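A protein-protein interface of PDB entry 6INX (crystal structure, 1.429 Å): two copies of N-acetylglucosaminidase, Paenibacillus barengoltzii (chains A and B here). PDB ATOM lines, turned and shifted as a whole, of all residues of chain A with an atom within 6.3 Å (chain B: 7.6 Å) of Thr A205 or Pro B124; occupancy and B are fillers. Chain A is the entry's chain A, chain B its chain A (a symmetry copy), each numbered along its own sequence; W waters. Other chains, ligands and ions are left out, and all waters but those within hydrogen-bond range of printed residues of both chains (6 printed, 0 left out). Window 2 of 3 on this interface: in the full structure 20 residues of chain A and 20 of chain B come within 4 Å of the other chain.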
ATOM      1  N   THR A 203      14.675 -16.692 -13.815  1.00  0.00           N
ATOM      2  CA  THR A 203      13.818 -15.819 -14.607  1.00  0.00           C
ATOM      3  C   THR A 203      12.448 -15.699 -13.950  1.00  0.00           C
ATOM      4  O   THR A 203      11.890 -16.682 -13.463  1.00  0.00           O
ATOM      5  CB  THR A 203      13.685 -16.379 -16.022  1.00  0.00           C
ATOM      6  OG1 THR A 203      14.995 -16.485 -16.599  1.00  0.00           O
ATOM      7  CG2 THR A 203      12.813 -15.477 -16.896  1.00  0.00           C
ATOM      8  N   GLY A 204      11.924 -14.481 -13.910  1.00  0.00           N
ATOM      9  CA  GLY A 204      10.648 -14.214 -13.274  1.00  0.00           C
ATOM     10  C   GLY A 204       9.488 -14.103 -14.246  1.00  0.00           C
ATOM     11  O   GLY A 204       9.643 -13.647 -15.379  1.00  0.00           O
ATOM     12  N   THR A 205       8.305 -14.493 -13.768  1.00  0.00           N
ATOM     13  CA  THR A 205       7.091 -14.368 -14.565  1.00  0.00           C
ATOM     14  C   THR A 205       6.763 -12.898 -14.796  1.00  0.00           C
ATOM     15  O   THR A 205       6.882 -12.062 -13.896  1.00  0.00           O
ATOM     16  CB  THR A 205       5.912 -15.086 -13.879  1.00  0.00           C
ATOM     17  OG1 THR A 205       4.751 -15.038 -14.725  1.00  0.00           O
ATOM     18  CG2 THR A 205       5.556 -14.437 -12.548  1.00  0.00           C
ATOM     19  N   GLY A 206       6.362 -12.577 -16.025  1.00  0.00           N
ATOM     20  CA  GLY A 206       5.976 -11.220 -16.347  1.00  0.00           C
ATOM     21  C   GLY A 206       7.083 -10.318 -16.845  1.00  0.00           C
ATOM     22  O   GLY A 206       6.812  -9.146 -17.113  1.00  0.00           O
ATOM     23  N   ASP A 207       8.317 -10.807 -16.943  1.00  0.00           N
ATOM     24  CA  ASP A 207       9.438 -10.047 -17.492  1.00  0.00           C
ATOM     25  C   ASP A 207       9.524 -10.297 -18.996  1.00  0.00           C
ATOM     26  O   ASP A 207       9.613 -11.448 -19.424  1.00  0.00           O
ATOM     27  CB  ASP A 207      10.733 -10.516 -16.822  1.00  0.00           C
ATOM     28  CG  ASP A 207      11.903  -9.583 -17.081  1.00  0.00           C
ATOM     29  OD1 ASP A 207      11.775  -8.679 -17.930  1.00  0.00           O
ATOM     30  OD2 ASP A 207      12.964  -9.771 -16.437  1.00  0.00           O
ATOM     31  N   ARG A 210      14.092 -12.515 -20.706  1.00  0.00           N
ATOM     32  CA  ARG A 210      13.984 -13.861 -20.148  1.00  0.00           C
ATOM     33  C   ARG A 210      15.293 -14.416 -19.591  1.00  0.00           C
ATOM     34  O   ARG A 210      15.325 -15.579 -19.182  1.00  0.00           O
ATOM     35  CB  ARG A 210      13.371 -14.828 -21.166  1.00  0.00           C
ATOM     36  CG  ARG A 210      12.071 -14.320 -21.812  1.00  0.00           C
ATOM     37  CD  ARG A 210      10.973 -14.013 -20.794  1.00  0.00           C
ATOM     38  NE  ARG A 210      10.524 -15.205 -20.091  1.00  0.00           N
ATOM     39  CZ  ARG A 210       9.928 -15.189 -18.903  1.00  0.00           C
ATOM     40  NH1 ARG A 210       9.711 -14.037 -18.278  1.00  0.00           N
ATOM     41  NH2 ARG A 210       9.568 -16.337 -18.340  1.00  0.00           N
ATOM     42  N   TYR A 252       9.362  -4.264 -13.634  1.00  0.00           N
ATOM     43  CA  TYR A 252       8.831  -4.434 -14.995  1.00  0.00           C
ATOM     44  C   TYR A 252       8.031  -3.212 -15.438  1.00  0.00           C
ATOM     45  O   TYR A 252       6.980  -3.324 -16.072  1.00  0.00           O
ATOM     46  CB  TYR A 252       8.076  -5.760 -15.196  1.00  0.00           C
ATOM     47  CG  TYR A 252       8.851  -6.934 -14.657  1.00  0.00           C
ATOM     48  CD1 TYR A 252      10.229  -6.999 -14.813  1.00  0.00           C
ATOM     49  CD2 TYR A 252       8.226  -7.946 -13.954  1.00  0.00           C
ATOM     50  CE1 TYR A 252      10.956  -8.047 -14.310  1.00  0.00           C
ATOM     51  CE2 TYR A 252       8.955  -9.005 -13.442  1.00  0.00           C
ATOM     52  CZ  TYR A 252      10.323  -9.038 -13.621  1.00  0.00           C
ATOM     53  OH  TYR A 252      11.078 -10.073 -13.108  1.00  0.00           O
ATOM     54  N   GLU A 285      10.495 -15.605  -6.757  1.00  0.00           N
ATOM     55  CA  GLU A 285      10.700 -16.444  -7.926  1.00  0.00           C
ATOM     56  C   GLU A 285      12.114 -16.292  -8.470  1.00  0.00           C
ATOM     57  O   GLU A 285      12.797 -17.287  -8.708  1.00  0.00           O
ATOM     58  CB  GLU A 285       9.675 -16.136  -9.021  1.00  0.00           C
ATOM     59  CG  GLU A 285       9.766 -17.131 -10.173  1.00  0.00           C
ATOM     60  CD  GLU A 285       8.695 -16.915 -11.227  1.00  0.00           C
ATOM     61  OE1 GLU A 285       8.072 -15.839 -11.225  1.00  0.00           O
ATOM     62  OE2 GLU A 285       8.484 -17.819 -12.059  1.00  0.00           O
ATOM     63  N   SER B  78      -6.788 -10.026 -18.517  1.00  0.00           N
ATOM     64  CA  SER B  78      -6.429 -10.911 -17.413  1.00  0.00           C
ATOM     65  C   SER B  78      -7.601 -11.065 -16.449  1.00  0.00           C
ATOM     66  O   SER B  78      -7.875 -12.163 -15.954  1.00  0.00           O
ATOM     67  CB  SER B  78      -5.188 -10.382 -16.688  1.00  0.00           C
ATOM     68  OG  SER B  78      -4.826 -11.189 -15.581  1.00  0.00           O
ATOM     69  N   PRO B 113      -0.712 -12.111 -22.461  1.00  0.00           N
ATOM     70  CA  PRO B 113      -0.929 -12.968 -21.286  1.00  0.00           C
ATOM     71  C   PRO B 113       0.340 -13.081 -20.450  1.00  0.00           C
ATOM     72  O   PRO B 113       1.414 -13.379 -20.978  1.00  0.00           O
ATOM     73  CB  PRO B 113      -1.304 -14.322 -21.903  1.00  0.00           C
ATOM     74  CG  PRO B 113      -1.896 -13.984 -23.241  1.00  0.00           C
ATOM     75  CD  PRO B 113      -1.112 -12.775 -23.720  1.00  0.00           C
ATOM     76  N   CYS B 114       0.217 -12.788 -19.145  1.00  0.00           N
ATOM     77  CA  CYS B 114       1.266 -12.814 -18.122  1.00  0.00           C
ATOM     78  C   CYS B 114       2.069 -11.520 -18.027  1.00  0.00           C
ATOM     79  O   CYS B 114       2.901 -11.395 -17.121  1.00  0.00           O
ATOM     80  CB  CYS B 114       2.236 -14.008 -18.240  1.00  0.00           C
ATOM     81  SG  CYS B 114       1.467 -15.650 -18.183  1.00  0.00           S
ATOM     82  N   TYR B 115       1.852 -10.565 -18.927  1.00  0.00           N
ATOM     83  CA  TYR B 115       2.689  -9.372 -19.033  1.00  0.00           C
ATOM     84  C   TYR B 115       1.869  -8.114 -18.786  1.00  0.00           C
ATOM     85  O   TYR B 115       0.853  -7.886 -19.449  1.00  0.00           O
ATOM     86  CB  TYR B 115       3.407  -9.333 -20.390  1.00  0.00           C
ATOM     87  CG  TYR B 115       4.312 -10.529 -20.515  1.00  0.00           C
ATOM     88  CD1 TYR B 115       5.532 -10.556 -19.855  1.00  0.00           C
ATOM     89  CD2 TYR B 115       3.922 -11.658 -21.221  1.00  0.00           C
ATOM     90  CE1 TYR B 115       6.355 -11.652 -19.917  1.00  0.00           C
ATOM     91  CE2 TYR B 115       4.743 -12.771 -21.290  1.00  0.00           C
ATOM     92  CZ  TYR B 115       5.959 -12.761 -20.631  1.00  0.00           C
ATOM     93  OH  TYR B 115       6.773 -13.875 -20.687  1.00  0.00           O
ATOM     94  N   GLU B 117       3.326  -4.977 -18.807  1.00  0.00           N
ATOM     95  CA  GLU B 117       4.171  -3.859 -19.203  1.00  0.00           C
ATOM     96  C   GLU B 117       3.405  -2.758 -19.927  1.00  0.00           C
ATOM     97  O   GLU B 117       3.863  -1.606 -19.937  1.00  0.00           O
ATOM     98  CB  GLU B 117       5.312  -4.362 -20.096  1.00  0.00           C
ATOM     99  CG  GLU B 117       6.500  -4.930 -19.349  1.00  0.00           C
ATOM    100  CD  GLU B 117       6.363  -6.383 -18.926  1.00  0.00           C
ATOM    101  OE1 GLU B 117       5.277  -6.977 -19.083  1.00  0.00           O
ATOM    102  OE2 GLU B 117       7.367  -6.906 -18.384  1.00  0.00           O
ATOM    103  N   ALA B 122      -2.135  -8.305 -15.092  1.00  0.00           N
ATOM    104  CA  ALA B 122      -1.575  -9.571 -15.540  1.00  0.00           C
ATOM    105  C   ALA B 122      -1.357 -10.473 -14.342  1.00  0.00           C
ATOM    106  O   ALA B 122      -1.290 -10.021 -13.193  1.00  0.00           O
ATOM    107  CB  ALA B 122      -0.234  -9.408 -16.273  1.00  0.00           C
ATOM    108  N   SER B 123      -1.198 -11.760 -14.635  1.00  0.00           N
ATOM    109  CA  SER B 123      -1.011 -12.765 -13.599  1.00  0.00           C
ATOM    110  C   SER B 123      -0.307 -13.963 -14.211  1.00  0.00           C
ATOM    111  O   SER B 123      -0.513 -14.257 -15.391  1.00  0.00           O
ATOM    112  CB  SER B 123      -2.373 -13.198 -13.040  1.00  0.00           C
ATOM    113  OG  SER B 123      -2.247 -14.389 -12.271  1.00  0.00           O
ATOM    114  N   PRO B 124       0.524 -14.678 -13.445  1.00  0.00           N
ATOM    115  CA  PRO B 124       1.030 -15.961 -13.951  1.00  0.00           C
ATOM    116  C   PRO B 124      -0.075 -16.911 -14.354  1.00  0.00           C
ATOM    117  O   PRO B 124       0.151 -17.780 -15.199  1.00  0.00           O
ATOM    118  CB  PRO B 124       1.837 -16.527 -12.772  1.00  0.00           C
ATOM    119  CG  PRO B 124       1.961 -15.433 -11.792  1.00  0.00           C
ATOM    120  CD  PRO B 124       0.921 -14.414 -12.051  1.00  0.00           C
ATOM    121  N   ASP B 125      -1.265 -16.783 -13.754  1.00  0.00           N
ATOM    122  CA  ASP B 125      -2.394 -17.625 -14.130  1.00  0.00           C
ATOM    123  C   ASP B 125      -2.848 -17.384 -15.564  1.00  0.00           C
ATOM    124  O   ASP B 125      -3.582 -18.216 -16.109  1.00  0.00           O
ATOM    125  CB  ASP B 125      -3.577 -17.393 -13.181  1.00  0.00           C
ATOM    126  CG  ASP B 125      -3.273 -17.791 -11.752  1.00  0.00           C
ATOM    127  OD1 ASP B 125      -2.363 -18.616 -11.541  1.00  0.00           O
ATOM    128  OD2 ASP B 125      -3.955 -17.276 -10.839  1.00  0.00           O
ATOM    129  N   ASP B 126      -2.428 -16.273 -16.189  1.00  0.00           N
ATOM    130  CA  ASP B 126      -2.849 -15.976 -17.558  1.00  0.00           C
ATOM    131  C   ASP B 126      -2.403 -17.057 -18.536  1.00  0.00           C
ATOM    132  O   ASP B 126      -3.027 -17.237 -19.587  1.00  0.00           O
ATOM    133  CB  ASP B 126      -2.253 -14.649 -18.038  1.00  0.00           C
ATOM    134  CG  ASP B 126      -2.756 -13.442 -17.290  1.00  0.00           C
ATOM    135  OD1 ASP B 126      -3.790 -13.507 -16.578  1.00  0.00           O
ATOM    136  OD2 ASP B 126      -2.101 -12.393 -17.452  1.00  0.00           O
ATOM    137  N   LYS B 127      -1.301 -17.746 -18.240  1.00  0.00           N
ATOM    138  CA  LYS B 127      -0.801 -18.749 -19.178  1.00  0.00           C
ATOM    139  C   LYS B 127      -1.829 -19.854 -19.402  1.00  0.00           C
ATOM    140  O   LYS B 127      -2.153 -20.195 -20.546  1.00  0.00           O
ATOM    141  CB  LYS B 127       0.529 -19.303 -18.667  1.00  0.00           C
ATOM    142  CG  LYS B 127       1.150 -20.349 -19.571  1.00  0.00           C
ATOM    143  CD  LYS B 127       2.587 -20.608 -19.170  1.00  0.00           C
ATOM    144  CE  LYS B 127       3.180 -21.752 -19.976  1.00  0.00           C
ATOM    145  NZ  LYS B 127       4.635 -21.880 -19.670  1.00  0.00           N
ATOM    146  N   ALA B 128      -2.378 -20.407 -18.321  1.00  0.00           N
ATOM    147  CA  ALA B 128      -3.438 -21.395 -18.478  1.00  0.00           C
ATOM    148  C   ALA B 128      -4.760 -20.740 -18.862  1.00  0.00           C
ATOM    149  O   ALA B 128      -5.513 -21.288 -19.677  1.00  0.00           O
ATOM    150  CB  ALA B 128      -3.587 -22.200 -17.183  1.00  0.00           C
ATOM    151  N   ASN B 129      -5.038 -19.545 -18.323  1.00  0.00           N
ATOM    152  CA  ASN B 129      -6.355 -18.936 -18.518  1.00  0.00           C
ATOM    153  C   ASN B 129      -6.566 -18.465 -19.956  1.00  0.00           C
ATOM    154  O   ASN B 129      -7.706 -18.434 -20.429  1.00  0.00           O
ATOM    155  CB  ASN B 129      -6.554 -17.772 -17.537  1.00  0.00           C
ATOM    156  CG  ASN B 129      -6.707 -18.238 -16.112  1.00  0.00           C
ATOM    157  OD1 ASN B 129      -6.935 -19.416 -15.862  1.00  0.00           O
ATOM    158  ND2 ASN B 129      -6.566 -17.327 -15.174  1.00  0.00           N
ATOM    159  N   ASP B 166       6.731 -18.062 -23.496  1.00  0.00           N
ATOM    160  CA  ASP B 166       6.815 -18.391 -22.081  1.00  0.00           C
ATOM    161  C   ASP B 166       5.535 -18.051 -21.334  1.00  0.00           C
ATOM    162  O   ASP B 166       5.283 -18.635 -20.277  1.00  0.00           O
ATOM    163  CB  ASP B 166       7.990 -17.652 -21.432  1.00  0.00           C
ATOM    164  CG  ASP B 166       9.343 -18.122 -21.950  1.00  0.00           C
ATOM    165  OD1 ASP B 166       9.395 -19.177 -22.618  1.00  0.00           O
ATOM    166  OD2 ASP B 166      10.354 -17.447 -21.670  1.00  0.00           O
ATOM    167  N   GLY B 167       4.723 -17.128 -21.849  1.00  0.00           N
ATOM    168  CA  GLY B 167       3.487 -16.756 -21.194  1.00  0.00           C
ATOM    169  C   GLY B 167       2.244 -17.421 -21.734  1.00  0.00           C
ATOM    170  O   GLY B 167       1.137 -17.072 -21.301  1.00  0.00           O
HETATM  171  O   HOH W   1       6.335 -14.807 -17.916  1.00  0.00           O
HETATM  172  O   HOH W   2      10.705 -19.056 -18.793  1.00  0.00           O
HETATM  173  O   HOH W   3       5.029 -17.243 -17.304  1.00  0.00           O
HETATM  174  O   HOH W   4       2.820 -12.728 -14.761  1.00  0.00           O
HETATM  175  O   HOH W   5       4.745  -4.936 -15.951  1.00  0.00           O
HETATM  176  O   HOH W   6       4.596  -7.757 -16.054  1.00  0.00           O
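The side-chain carboxylate of Glu B117 lies close to the backbone carbonyl oxygen of Gly A206. The guanidinium group (NE) of Arg A210 is in salt-bridge range of the side-chain carboxylate (OD2) of Asp B166.
The side-chain hydroxyl of Thr A203 lies within hydrogen-bond range of the backbone carbonyl oxygen of Arg A210. The backbone carbonyl oxygen (O) of Gly A204 is in hydrogen-bond range of the guanidinium group (NH1) of Arg A210, 2.9 Å away. O of Asp A207 lies within hydrogen-bond range of NH1 of Arg A210, 2.8 Å away. The backbone NH (N) of Cys B114 sits at hydrogen-bond distance from the side-chain carboxylate (OD2) of Asp B126, at 2.9 Å. The side-chain sulfur (SG) of Cys B114 lies within hydrogen-bond range of the backbone NH (N) of Lys B127. The backbone carbonyl oxygen (O) of Gly B167 lies within hydrogen-bond range of the side-chain sulfur (SG) of Cys B114, at 3.4 Å.
Among the printed residues, merely in contact across the chains: Gly A206 with Cys B114, Asp A207 with Tyr B115, Gly A206 with Tyr B115, Tyr A252 with Glu B117, Arg A210 with Tyr B115, Thr A205 with Pro B124 and Asp A207 with Glu B117.
Gly A204 touches none of the printed residues of chain B. Of chain B, only Pro B124 comes within 4 Å of Thr A205. Printed residues of chain B within 4 Å of Gly A206: Cys B114, Tyr B115 and Glu B117. Of the printed residues of chain A, Tyr B115 touches Gly A206, Asp A207 and Arg A210. Of the printed residues of chain A, Glu B117 touches Gly A206 (2.6 Å), Asp A207 (3.9 Å) and Tyr A252 (3.5 Å). Ala B122 touches none of the printed residues of chain A. Pro B124 touches just one residue of chain A: Thr A205.
Of the 8 printed residues of chain A, 5 touch a printed residue of chain B. Among the printed residues, 9 pairs touch across the chains. Among the printed residues, Asp or Glu carboxylates within 4 Å of a Lys or Arg side-chain nitrogen of the other chain: Arg A210 with Asp B166 (2.7 Å).
No position is printed for both chains.
Water W4 bridges the backbone carbonyl oxygen (O) of Cys B114 (2.7 Å) and the side-chain hydroxyl (OG1) of Thr A205 (3.0 Å). Water W5 lies within hydrogen-bond range of the backbone carbonyl oxygen of Tyr A252 and the backbone NH of Glu B117. Water W6 bridges O of Gly A206 (2.8 Å) and OE1 of Glu B117 (3.2 Å). Water W1 lies within hydrogen-bond range of N of Gly A206 (2.9 Å), OH of Tyr B115 (3.0 Å) and NH1 of Arg A210 (3.5 Å). Water W2 lies within hydrogen-bond range of the guanidinium group of Arg A210 (3.0 Å) and the side-chain carboxylate of Asp B166 (3.3 Å). Water W3 lies within hydrogen-bond range of the backbone carbonyl oxygen of Asp B166 (3.3 Å) and the side-chain hydroxyl of Thr A205 (3.4 Å).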
